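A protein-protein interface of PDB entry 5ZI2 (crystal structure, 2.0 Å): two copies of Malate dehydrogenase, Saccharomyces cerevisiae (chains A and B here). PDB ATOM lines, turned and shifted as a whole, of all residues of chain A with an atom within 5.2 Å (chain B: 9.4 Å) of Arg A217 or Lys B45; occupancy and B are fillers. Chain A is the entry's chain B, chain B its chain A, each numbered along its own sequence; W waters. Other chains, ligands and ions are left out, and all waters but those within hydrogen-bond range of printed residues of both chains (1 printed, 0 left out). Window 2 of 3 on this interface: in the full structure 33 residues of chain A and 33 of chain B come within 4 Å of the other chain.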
ATOM      1  N   PHE A 158      12.459  -8.983  -9.302  1.00  0.00           N
ATOM      2  CA  PHE A 158      13.503  -9.958  -9.104  1.00  0.00           C
ATOM      3  C   PHE A 158      13.691 -10.836 -10.329  1.00  0.00           C
ATOM      4  O   PHE A 158      14.819 -11.283 -10.632  1.00  0.00           O
ATOM      5  CB  PHE A 158      13.238 -10.832  -7.903  1.00  0.00           C
ATOM      6  CG  PHE A 158      13.055 -10.104  -6.636  1.00  0.00           C
ATOM      7  CD1 PHE A 158      13.646  -8.879  -6.399  1.00  0.00           C
ATOM      8  CD2 PHE A 158      12.390 -10.716  -5.601  1.00  0.00           C
ATOM      9  CE1 PHE A 158      13.491  -8.254  -5.191  1.00  0.00           C
ATOM     10  CE2 PHE A 158      12.216 -10.081  -4.398  1.00  0.00           C
ATOM     11  CZ  PHE A 158      12.776  -8.852  -4.196  1.00  0.00           C
ATOM     12  N   ASP A 161      16.014  -8.806 -12.258  1.00  0.00           N
ATOM     13  CA  ASP A 161      17.337  -8.774 -11.606  1.00  0.00           C
ATOM     14  C   ASP A 161      18.103 -10.086 -11.826  1.00  0.00           C
ATOM     15  O   ASP A 161      19.322 -10.051 -12.028  1.00  0.00           O
ATOM     16  CB  ASP A 161      17.263  -8.518 -10.090  1.00  0.00           C
ATOM     17  CG  ASP A 161      16.687  -7.119  -9.729  1.00  0.00           C
ATOM     18  OD1 ASP A 161      16.563  -6.201 -10.577  1.00  0.00           O
ATOM     19  OD2 ASP A 161      16.354  -6.934  -8.549  1.00  0.00           O
ATOM     20  N   TYR A 162      17.415 -11.232 -11.730  1.00  0.00           N
ATOM     21  CA  TYR A 162      18.112 -12.511 -11.867  1.00  0.00           C
ATOM     22  C   TYR A 162      18.476 -12.769 -13.299  1.00  0.00           C
ATOM     23  O   TYR A 162      19.539 -13.264 -13.519  1.00  0.00           O
ATOM     24  CB  TYR A 162      17.383 -13.695 -11.264  1.00  0.00           C
ATOM     25  CG  TYR A 162      17.508 -13.817  -9.756  1.00  0.00           C
ATOM     26  CD1 TYR A 162      18.659 -14.355  -9.175  1.00  0.00           C
ATOM     27  CD2 TYR A 162      16.455 -13.483  -8.919  1.00  0.00           C
ATOM     28  CE1 TYR A 162      18.778 -14.507  -7.787  1.00  0.00           C
ATOM     29  CE2 TYR A 162      16.574 -13.605  -7.534  1.00  0.00           C
ATOM     30  CZ  TYR A 162      17.732 -14.128  -6.977  1.00  0.00           C
ATOM     31  OH  TYR A 162      17.841 -14.249  -5.587  1.00  0.00           O
ATOM     32  N   GLU A 212      15.488 -21.469  -8.201  1.00  0.00           N
ATOM     33  CA  GLU A 212      15.154 -21.581  -6.762  1.00  0.00           C
ATOM     34  C   GLU A 212      15.521 -20.388  -5.887  1.00  0.00           C
ATOM     35  O   GLU A 212      14.831 -20.080  -4.900  1.00  0.00           O
ATOM     36  CB  GLU A 212      15.739 -22.852  -6.156  1.00  0.00           C
ATOM     37  CG  GLU A 212      15.123 -24.120  -6.728  1.00  0.00           C
ATOM     38  CD  GLU A 212      13.713 -24.394  -6.234  1.00  0.00           C
ATOM     39  OE1 GLU A 212      13.350 -23.937  -5.099  1.00  0.00           O
ATOM     40  OE2 GLU A 212      12.985 -25.104  -6.985  1.00  0.00           O
ATOM     41  N   HIS A 213      16.621 -19.738  -6.200  1.00  0.00           N
ATOM     42  CA  HIS A 213      16.969 -18.516  -5.554  1.00  0.00           C
ATOM     43  C   HIS A 213      15.863 -17.469  -5.806  1.00  0.00           C
ATOM     44  O   HIS A 213      15.513 -16.745  -4.893  1.00  0.00           O
ATOM     45  CB  HIS A 213      18.297 -17.965  -6.076  1.00  0.00           C
ATOM     46  CG  HIS A 213      19.496 -18.654  -5.525  1.00  0.00           C
ATOM     47  ND1 HIS A 213      20.398 -19.325  -6.326  1.00  0.00           N
ATOM     48  CD2 HIS A 213      19.938 -18.795  -4.252  1.00  0.00           C
ATOM     49  CE1 HIS A 213      21.346 -19.845  -5.567  1.00  0.00           C
ATOM     50  NE2 HIS A 213      21.093 -19.532  -4.307  1.00  0.00           N
ATOM     51  N   PHE A 214      15.355 -17.381  -7.039  1.00  0.00           N
ATOM     52  CA  PHE A 214      14.302 -16.454  -7.365  1.00  0.00           C
ATOM     53  C   PHE A 214      13.080 -16.691  -6.491  1.00  0.00           C
ATOM     54  O   PHE A 214      12.539 -15.739  -5.883  1.00  0.00           O
ATOM     55  CB  PHE A 214      13.986 -16.478  -8.846  1.00  0.00           C
ATOM     56  CG  PHE A 214      12.659 -15.893  -9.200  1.00  0.00           C
ATOM     57  CD1 PHE A 214      12.486 -14.539  -9.316  1.00  0.00           C
ATOM     58  CD2 PHE A 214      11.590 -16.699  -9.452  1.00  0.00           C
ATOM     59  CE1 PHE A 214      11.237 -14.010  -9.680  1.00  0.00           C
ATOM     60  CE2 PHE A 214      10.364 -16.198  -9.803  1.00  0.00           C
ATOM     61  CZ  PHE A 214      10.173 -14.857  -9.906  1.00  0.00           C
ATOM     62  N   ILE A 215      12.690 -17.956  -6.379  1.00  0.00           N
ATOM     63  CA  ILE A 215      11.494 -18.351  -5.647  1.00  0.00           C
ATOM     64  C   ILE A 215      11.686 -17.962  -4.228  1.00  0.00           C
ATOM     65  O   ILE A 215      10.756 -17.388  -3.659  1.00  0.00           O
ATOM     66  CB  ILE A 215      11.182 -19.878  -5.656  1.00  0.00           C
ATOM     67  CG1 ILE A 215      10.305 -20.256  -6.871  1.00  0.00           C
ATOM     68  CG2 ILE A 215      10.319 -20.275  -4.429  1.00  0.00           C
ATOM     69  CD1 ILE A 215      11.042 -20.317  -8.134  1.00  0.00           C
ATOM     70  N   HIS A 216      12.854 -18.304  -3.653  1.00  0.00           N
ATOM     71  CA  HIS A 216      13.167 -17.926  -2.263  1.00  0.00           C
ATOM     72  C   HIS A 216      13.141 -16.392  -2.100  1.00  0.00           C
ATOM     73  O   HIS A 216      12.638 -15.884  -1.114  1.00  0.00           O
ATOM     74  CB  HIS A 216      14.505 -18.543  -1.767  1.00  0.00           C
ATOM     75  CG  HIS A 216      14.838 -18.227  -0.333  1.00  0.00           C
ATOM     76  ND1 HIS A 216      14.332 -18.946   0.733  1.00  0.00           N
ATOM     77  CD2 HIS A 216      15.645 -17.285   0.209  1.00  0.00           C
ATOM     78  CE1 HIS A 216      14.776 -18.438   1.870  1.00  0.00           C
ATOM     79  NE2 HIS A 216      15.598 -17.443   1.579  1.00  0.00           N
ATOM     80  N   ARG A 217      13.677 -15.648  -3.055  1.00  0.00           N
ATOM     81  CA  ARG A 217      13.741 -14.230  -2.837  1.00  0.00           C
ATOM     82  C   ARG A 217      12.345 -13.532  -2.813  1.00  0.00           C
ATOM     83  O   ARG A 217      12.075 -12.654  -1.984  1.00  0.00           O
ATOM     84  CB  ARG A 217      14.660 -13.586  -3.828  1.00  0.00           C
ATOM     85  CG  ARG A 217      15.175 -12.278  -3.279  1.00  0.00           C
ATOM     86  CD  ARG A 217      15.906 -11.567  -4.363  1.00  0.00           C
ATOM     87  NE  ARG A 217      16.304 -10.283  -3.863  1.00  0.00           N
ATOM     88  CZ  ARG A 217      16.681  -9.291  -4.648  1.00  0.00           C
ATOM     89  NH1 ARG A 217      16.774  -9.452  -5.962  1.00  0.00           N
ATOM     90  NH2 ARG A 217      16.992  -8.128  -4.104  1.00  0.00           N
ATOM     91  N   VAL A 218      11.439 -13.965  -3.686  1.00  0.00           N
ATOM     92  CA  VAL A 218      10.052 -13.438  -3.660  1.00  0.00           C
ATOM     93  C   VAL A 218       9.413 -13.861  -2.332  1.00  0.00           C
ATOM     94  O   VAL A 218       8.791 -13.071  -1.639  1.00  0.00           O
ATOM     95  CB  VAL A 218       9.254 -14.015  -4.816  1.00  0.00           C
ATOM     96  CG1 VAL A 218       7.796 -13.638  -4.693  1.00  0.00           C
ATOM     97  CG2 VAL A 218       9.842 -13.604  -6.122  1.00  0.00           C
ATOM     98  N   GLN A 219       9.581 -15.115  -1.941  1.00  0.00           N
ATOM     99  CA  GLN A 219       8.999 -15.572  -0.663  1.00  0.00           C
ATOM    100  C   GLN A 219       9.484 -14.813   0.568  1.00  0.00           C
ATOM    101  O   GLN A 219       8.705 -14.517   1.491  1.00  0.00           O
ATOM    102  CB  GLN A 219       9.208 -17.086  -0.471  1.00  0.00           C
ATOM    103  CG  GLN A 219       8.400 -17.949  -1.478  1.00  0.00           C
ATOM    104  CD  GLN A 219       8.616 -19.433  -1.274  1.00  0.00           C
ATOM    105  OE1 GLN A 219       9.714 -19.843  -0.851  1.00  0.00           O
ATOM    106  NE2 GLN A 219       7.574 -20.247  -1.522  1.00  0.00           N
ATOM    107  N   PHE A 220      10.766 -14.502   0.617  1.00  0.00           N
ATOM    108  CA  PHE A 220      11.315 -13.881   1.823  1.00  0.00           C
ATOM    109  C   PHE A 220      11.766 -12.440   1.589  1.00  0.00           C
ATOM    110  O   PHE A 220      12.600 -11.931   2.304  1.00  0.00           O
ATOM    111  CB  PHE A 220      12.392 -14.820   2.367  1.00  0.00           C
ATOM    112  CG  PHE A 220      11.794 -16.111   2.872  1.00  0.00           C
ATOM    113  CD1 PHE A 220      11.291 -16.184   4.165  1.00  0.00           C
ATOM    114  CD2 PHE A 220      11.599 -17.182   2.018  1.00  0.00           C
ATOM    115  CE1 PHE A 220      10.660 -17.353   4.623  1.00  0.00           C
ATOM    116  CE2 PHE A 220      10.974 -18.353   2.461  1.00  0.00           C
ATOM    117  CZ  PHE A 220      10.528 -18.438   3.763  1.00  0.00           C
ATOM    118  N   GLY A 221      11.115 -11.764   0.626  1.00  0.00           N
ATOM    119  CA  GLY A 221      11.410 -10.377   0.273  1.00  0.00           C
ATOM    120  C   GLY A 221      11.346  -9.383   1.405  1.00  0.00           C
ATOM    121  O   GLY A 221      12.189  -8.508   1.488  1.00  0.00           O
ATOM    122  N   GLU A 224      14.433  -9.301   3.638  1.00  0.00           N
ATOM    123  CA  GLU A 224      15.505  -8.506   3.043  1.00  0.00           C
ATOM    124  C   GLU A 224      15.446  -6.998   3.442  1.00  0.00           C
ATOM    125  O   GLU A 224      16.489  -6.353   3.575  1.00  0.00           O
ATOM    126  CB  GLU A 224      15.399  -8.684   1.554  1.00  0.00           C
ATOM    127  CG  GLU A 224      16.461  -8.104   0.684  1.00  0.00           C
ATOM    128  CD  GLU A 224      16.134  -8.401  -0.781  1.00  0.00           C
ATOM    129  OE1 GLU A 224      15.958  -9.574  -1.137  1.00  0.00           O
ATOM    130  OE2 GLU A 224      16.086  -7.463  -1.617  1.00  0.00           O
ATOM    131  N   ILE A 225      14.243  -6.463   3.667  1.00  0.00           N
ATOM    132  CA  ILE A 225      14.115  -5.056   4.014  1.00  0.00           C
ATOM    133  C   ILE A 225      14.303  -4.897   5.512  1.00  0.00           C
ATOM    134  O   ILE A 225      14.959  -3.955   5.972  1.00  0.00           O
ATOM    135  CB  ILE A 225      12.732  -4.497   3.628  1.00  0.00           C
ATOM    136  CG1 ILE A 225      12.413  -4.763   2.133  1.00  0.00           C
ATOM    137  CG2 ILE A 225      12.624  -3.010   4.008  1.00  0.00           C
ATOM    138  CD1 ILE A 225      13.475  -4.274   1.221  1.00  0.00           C
ATOM    139  N   ALA A 228      17.873  -4.983   5.889  1.00  0.00           N
ATOM    140  CA  ALA A 228      18.472  -3.724   5.417  1.00  0.00           C
ATOM    141  C   ALA A 228      18.238  -2.518   6.384  1.00  0.00           C
ATOM    142  O   ALA A 228      19.066  -1.608   6.439  1.00  0.00           O
ATOM    143  CB  ALA A 228      17.979  -3.403   4.014  1.00  0.00           C
ATOM    144  N   SER B  20      12.033  10.394  -2.827  1.00  0.00           N
ATOM    145  CA  SER B  20      12.717   9.237  -3.349  1.00  0.00           C
ATOM    146  C   SER B  20      11.769   8.220  -3.998  1.00  0.00           C
ATOM    147  O   SER B  20      12.085   7.689  -5.038  1.00  0.00           O
ATOM    148  CB  SER B  20      13.594   8.553  -2.286  1.00  0.00           C
ATOM    149  OG  SER B  20      14.513   9.519  -1.715  1.00  0.00           O
ATOM    150  N   LYS B  24      11.826   7.121  -7.897  1.00  0.00           N
ATOM    151  CA  LYS B  24      11.886   5.736  -8.300  1.00  0.00           C
ATOM    152  C   LYS B  24      10.887   5.396  -9.437  1.00  0.00           C
ATOM    153  O   LYS B  24      11.196   4.580 -10.254  1.00  0.00           O
ATOM    154  CB  LYS B  24      11.684   4.806  -7.111  1.00  0.00           C
ATOM    155  CG  LYS B  24      11.756   3.288  -7.426  1.00  0.00           C
ATOM    156  CD  LYS B  24      13.198   2.876  -7.740  1.00  0.00           C
ATOM    157  CE  LYS B  24      13.336   1.399  -8.122  1.00  0.00           C
ATOM    158  NZ  LYS B  24      13.116   1.084  -9.567  1.00  0.00           N
ATOM    159  N   LEU B  32      19.159   5.628  -9.359  1.00  0.00           N
ATOM    160  CA  LEU B  32      18.775   6.542  -8.327  1.00  0.00           C
ATOM    161  C   LEU B  32      19.656   6.240  -7.136  1.00  0.00           C
ATOM    162  O   LEU B  32      19.653   5.089  -6.664  1.00  0.00           O
ATOM    163  CB  LEU B  32      17.316   6.289  -7.959  1.00  0.00           C
ATOM    164  CG  LEU B  32      16.673   7.160  -6.866  1.00  0.00           C
ATOM    165  CD1 LEU B  32      16.876   8.637  -7.114  1.00  0.00           C
ATOM    166  CD2 LEU B  32      15.204   6.794  -6.674  1.00  0.00           C
ATOM    167  N   LEU B  34      20.658   7.148  -3.181  1.00  0.00           N
ATOM    168  CA  LEU B  34      20.109   7.874  -2.044  1.00  0.00           C
ATOM    169  C   LEU B  34      21.166   7.993  -0.972  1.00  0.00           C
ATOM    170  O   LEU B  34      21.821   7.049  -0.687  1.00  0.00           O
ATOM    171  CB  LEU B  34      18.909   7.173  -1.494  1.00  0.00           C
ATOM    172  CG  LEU B  34      17.808   6.768  -2.477  1.00  0.00           C
ATOM    173  CD1 LEU B  34      16.661   6.106  -1.737  1.00  0.00           C
ATOM    174  CD2 LEU B  34      17.302   8.008  -3.275  1.00  0.00           C
ATOM    175  N   ALA B  39      19.955   5.931   7.589  1.00  0.00           N
ATOM    176  CA  ALA B  39      18.848   5.148   7.115  1.00  0.00           C
ATOM    177  C   ALA B  39      18.681   5.039   5.577  1.00  0.00           C
ATOM    178  O   ALA B  39      17.733   4.364   5.148  1.00  0.00           O
ATOM    179  CB  ALA B  39      17.538   5.616   7.748  1.00  0.00           C
ATOM    180  N   ALA B  40      19.601   5.600   4.784  1.00  0.00           N
ATOM    181  CA  ALA B  40      19.380   5.614   3.318  1.00  0.00           C
ATOM    182  C   ALA B  40      19.521   4.253   2.726  1.00  0.00           C
ATOM    183  O   ALA B  40      18.843   4.005   1.753  1.00  0.00           O
ATOM    184  CB  ALA B  40      20.267   6.604   2.547  1.00  0.00           C
ATOM    185  N   GLU B  41      20.418   3.402   3.261  1.00  0.00           N
ATOM    186  CA  GLU B  41      20.558   2.057   2.731  1.00  0.00           C
ATOM    187  C   GLU B  41      19.236   1.273   2.735  1.00  0.00           C
ATOM    188  O   GLU B  41      18.932   0.640   1.788  1.00  0.00           O
ATOM    189  CB  GLU B  41      21.614   1.241   3.497  1.00  0.00           C
ATOM    190  CG  GLU B  41      23.008   1.716   3.181  1.00  0.00           C
ATOM    191  CD  GLU B  41      24.054   1.248   4.201  1.00  0.00           C
ATOM    192  OE1 GLU B  41      23.940   1.597   5.396  1.00  0.00           O
ATOM    193  OE2 GLU B  41      25.011   0.597   3.775  1.00  0.00           O
ATOM    194  N   GLY B  42      18.519   1.366   3.828  1.00  0.00           N
ATOM    195  CA  GLY B  42      17.278   0.668   4.035  1.00  0.00           C
ATOM    196  C   GLY B  42      16.132   1.189   3.204  1.00  0.00           C
ATOM    197  O   GLY B  42      15.345   0.392   2.713  1.00  0.00           O
ATOM    198  N   ILE B  43      16.085   2.496   2.991  1.00  0.00           N
ATOM    199  CA  ILE B  43      15.063   3.085   2.111  1.00  0.00           C
ATOM    200  C   ILE B  43      15.332   2.761   0.673  1.00  0.00           C
ATOM    201  O   ILE B  43      14.374   2.448  -0.067  1.00  0.00           O
ATOM    202  CB  ILE B  43      14.982   4.582   2.358  1.00  0.00           C
ATOM    203  CG1 ILE B  43      14.381   4.799   3.771  1.00  0.00           C
ATOM    204  CG2 ILE B  43      14.163   5.289   1.256  1.00  0.00           C
ATOM    205  CD1 ILE B  43      14.854   6.075   4.445  1.00  0.00           C
ATOM    206  N   GLY B  44      16.613   2.797   0.266  1.00  0.00           N
ATOM    207  CA  GLY B  44      17.001   2.402  -1.070  1.00  0.00           C
ATOM    208  C   GLY B  44      16.660   0.974  -1.341  1.00  0.00           C
ATOM    209  O   GLY B  44      16.244   0.622  -2.441  1.00  0.00           O
ATOM    210  N   LYS B  45      16.894   0.116  -0.341  1.00  0.00           N
ATOM    211  CA  LYS B  45      16.569  -1.276  -0.528  1.00  0.00           C
ATOM    212  C   LYS B  45      15.054  -1.520  -0.689  1.00  0.00           C
ATOM    213  O   LYS B  45      14.647  -2.263  -1.563  1.00  0.00           O
ATOM    214  CB  LYS B  45      17.118  -2.130   0.617  1.00  0.00           C
ATOM    215  CG  LYS B  45      17.268  -3.597   0.253  1.00  0.00           C
ATOM    216  CD  LYS B  45      18.491  -3.795  -0.622  1.00  0.00           C
ATOM    217  CE  LYS B  45      18.781  -5.273  -0.815  1.00  0.00           C
ATOM    218  NZ  LYS B  45      19.306  -5.480  -2.202  1.00  0.00           N
ATOM    219  N   ASP B  46      14.260  -0.920   0.175  1.00  0.00           N
ATOM    220  CA  ASP B  46      12.776  -0.877   0.057  1.00  0.00           C
ATOM    221  C   ASP B  46      12.375  -0.520  -1.382  1.00  0.00           C
ATOM    222  O   ASP B  46      11.650  -1.261  -2.088  1.00  0.00           O
ATOM    223  CB  ASP B  46      12.282   0.239   1.037  1.00  0.00           C
ATOM    224  CG  ASP B  46      10.783   0.235   1.286  1.00  0.00           C
ATOM    225  OD1 ASP B  46      10.065  -0.326   0.475  1.00  0.00           O
ATOM    226  OD2 ASP B  46      10.320   0.754   2.340  1.00  0.00           O
ATOM    227  N   LEU B  47      12.857   0.633  -1.823  1.00  0.00           N
ATOM    228  CA  LEU B  47      12.538   1.173  -3.124  1.00  0.00           C
ATOM    229  C   LEU B  47      12.980   0.299  -4.270  1.00  0.00           C
ATOM    230  O   LEU B  47      12.298   0.249  -5.310  1.00  0.00           O
ATOM    231  CB  LEU B  47      13.098   2.595  -3.262  1.00  0.00           C
ATOM    232  CG  LEU B  47      12.324   3.619  -2.444  1.00  0.00           C
ATOM    233  CD1 LEU B  47      13.034   4.976  -2.433  1.00  0.00           C
ATOM    234  CD2 LEU B  47      10.874   3.763  -2.958  1.00  0.00           C
ATOM    235  N   SER B  48      14.091  -0.407  -4.083  1.00  0.00           N
ATOM    236  CA  SER B  48      14.669  -1.235  -5.116  1.00  0.00           C
ATOM    237  C   SER B  48      13.743  -2.417  -5.473  1.00  0.00           C
ATOM    238  O   SER B  48      13.876  -2.928  -6.562  1.00  0.00           O
ATOM    239  CB  SER B  48      16.032  -1.830  -4.741  1.00  0.00           C
ATOM    240  OG  SER B  48      15.922  -2.880  -3.777  1.00  0.00           O
ATOM    241  N   HIS B  49      12.799  -2.756  -4.613  1.00  0.00           N
ATOM    242  CA  HIS B  49      11.815  -3.842  -4.913  1.00  0.00           C
ATOM    243  C   HIS B  49      10.725  -3.390  -5.886  1.00  0.00           C
ATOM    244  O   HIS B  49      10.087  -4.232  -6.460  1.00  0.00           O
ATOM    245  CB  HIS B  49      11.198  -4.343  -3.653  1.00  0.00           C
ATOM    246  CG  HIS B  49      12.147  -5.090  -2.791  1.00  0.00           C
ATOM    247  ND1 HIS B  49      11.734  -5.824  -1.700  1.00  0.00           N
ATOM    248  CD2 HIS B  49      13.485  -5.298  -2.905  1.00  0.00           C
ATOM    249  CE1 HIS B  49      12.776  -6.439  -1.164  1.00  0.00           C
ATOM    250  NE2 HIS B  49      13.844  -6.144  -1.886  1.00  0.00           N
ATOM    251  N   ILE B  50      10.511  -2.089  -6.008  1.00  0.00           N
ATOM    252  CA  ILE B  50       9.487  -1.521  -6.921  1.00  0.00           C
ATOM    253  C   ILE B  50       9.834  -1.859  -8.350  1.00  0.00           C
ATOM    254  O   ILE B  50      10.930  -1.593  -8.777  1.00  0.00           O
ATOM    255  CB  ILE B  50       9.370   0.002  -6.770  1.00  0.00           C
ATOM    256  CG1 ILE B  50       8.804   0.329  -5.372  1.00  0.00           C
ATOM    257  CG2 ILE B  50       8.535   0.643  -7.873  1.00  0.00           C
ATOM    258  CD1 ILE B  50       8.715   1.779  -5.056  1.00  0.00           C
ATOM    259  N   SER B  55      17.740   1.423 -11.322  1.00  0.00           N
ATOM    260  CA  SER B  55      18.343   0.690 -10.205  1.00  0.00           C
ATOM    261  C   SER B  55      18.398   1.726  -9.051  1.00  0.00           C
ATOM    262  O   SER B  55      18.630   2.877  -9.307  1.00  0.00           O
ATOM    263  CB  SER B  55      19.728   0.149 -10.541  1.00  0.00           C
ATOM    264  OG  SER B  55      20.624   1.235 -10.533  1.00  0.00           O
ATOM    265  N   CYS B  56      18.150   1.311  -7.819  1.00  0.00           N
ATOM    266  CA  CYS B  56      18.070   2.210  -6.703  1.00  0.00           C
ATOM    267  C   CYS B  56      18.899   1.637  -5.592  1.00  0.00           C
ATOM    268  O   CYS B  56      18.606   0.528  -5.136  1.00  0.00           O
ATOM    269  CB  CYS B  56      16.613   2.323  -6.197  1.00  0.00           C
ATOM    270  SG  CYS B  56      16.468   3.455  -4.784  1.00  0.00           S
ATOM    271  N   VAL B  57      19.868   2.399  -5.123  1.00  0.00           N
ATOM    272  CA  VAL B  57      20.769   1.990  -4.051  1.00  0.00           C
ATOM    273  C   VAL B  57      20.885   3.135  -3.071  1.00  0.00           C
ATOM    274  O   VAL B  57      21.031   4.258  -3.518  1.00  0.00           O
ATOM    275  CB  VAL B  57      22.205   1.714  -4.589  1.00  0.00           C
ATOM    276  CG1 VAL B  57      23.160   1.349  -3.424  1.00  0.00           C
ATOM    277  CG2 VAL B  57      22.221   0.649  -5.694  1.00  0.00           C
ATOM    278  N   GLY B  58      20.816   2.854  -1.772  1.00  0.00           N
ATOM    279  CA  GLY B  58      21.044   3.847  -0.722  1.00  0.00           C
ATOM    280  C   GLY B  58      22.425   3.698  -0.088  1.00  0.00           C
ATOM    281  O   GLY B  58      22.995   2.631  -0.074  1.00  0.00           O
ATOM    282  N   TYR B  59      22.958   4.780   0.393  1.00  0.00           N
ATOM    283  CA  TYR B  59      24.356   4.816   0.854  1.00  0.00           C
ATOM    284  C   TYR B  59      24.428   5.337   2.266  1.00  0.00           C
ATOM    285  O   TYR B  59      23.638   6.204   2.649  1.00  0.00           O
ATOM    286  CB  TYR B  59      25.143   5.734  -0.037  1.00  0.00           C
ATOM    287  CG  TYR B  59      25.315   5.156  -1.382  1.00  0.00           C
ATOM    288  CD1 TYR B  59      24.340   5.335  -2.365  1.00  0.00           C
ATOM    289  CD2 TYR B  59      26.376   4.301  -1.642  1.00  0.00           C
ATOM    290  CE1 TYR B  59      24.469   4.779  -3.621  1.00  0.00           C
ATOM    291  CE2 TYR B  59      26.535   3.737  -2.878  1.00  0.00           C
ATOM    292  CZ  TYR B  59      25.596   3.995  -3.870  1.00  0.00           C
ATOM    293  OH  TYR B  59      25.740   3.409  -5.078  1.00  0.00           O
HETATM  294  O   HOH W   1      17.408  -5.032  -4.342  1.00  0.00           O
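Among the printed residues, pairs that only touch across the chains: Ile A225 with His B49, Gly A221 with His B49, Ile A225 with Asp B46, Ile A225 with Lys B45, Phe A158 with His B49, Ala A228 with Lys B45, Ala A228 with Gly B42 and Arg A217 with Lys B45.
No position is printed for both chains.
Water W1 lies within hydrogen-bond range of the side-chain hydroxyl of Ser B48 (2.7 Å), the side-chain amino group of Lys B45 (2.9 Å) and the guanidinium group of Arg A217 (3.1 Å).
The backbone carbonyl oxygen of Lys B45 lies within hydrogen-bond range of the side-chain hydroxyl of Ser B48, 2.6 Å away.
NH1 of Arg A217 lies within salt-bridge range of OD2 of Asp A161 (3.6 Å).
The guanidinium group (NH2) of Arg A217 lies within salt-bridge range of the side-chain carboxylate (OE2) of Glu A224 (2.7 Å).
Hydrophobic or aromatic side chains of chain B within 4 Å of the printed part of chain A: His B49.
Along chain B the printed residues that touch a printed residue of chain A span positions 42 to 49.
Of the 16 printed residues of chain A, 6 touch a printed residue of chain B.
Printed residues of chain A that touch a printed residue of chain B: Phe A158, Arg A217, Gly A221, Glu A224, Ile A225 and Ala A228.
Among the printed residues, Asp or Glu carboxylates within 4 Å of a Lys or Arg side-chain nitrogen of the other chain: Glu A224 with Lys B45.
Of the printed residues of chain B, Arg A217 touches Lys B45 (3.998 Å).
Of the printed residues of chain A, Lys B45 touches Arg A217, Glu A224, Ile A225 and Ala A228.
No residue of chain B comes within 4 Å of Val A218.
Of the printed residues of chain B, Gly A221 touches His B49.
Printed residues of chain B within 4 Å of Phe A158: His B49.
Printed residues of chain A within 4 Å of Asp B46: Ile A225 (3.6 Å).
Of the printed residues of chain B, Glu A224 touches Lys B45 and His B49.
Leu B47 touches none of the printed residues of chain A.
The side-chain amino group of Lys B45 is in salt-bridge range of the side-chain carboxylate of Glu A224, at 3.8 Å.
The side-chain carboxylate (OE2) of Glu A224 sits at hydrogen-bond distance from a ring nitrogen (NE2) of His B49, at 2.6 Å.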
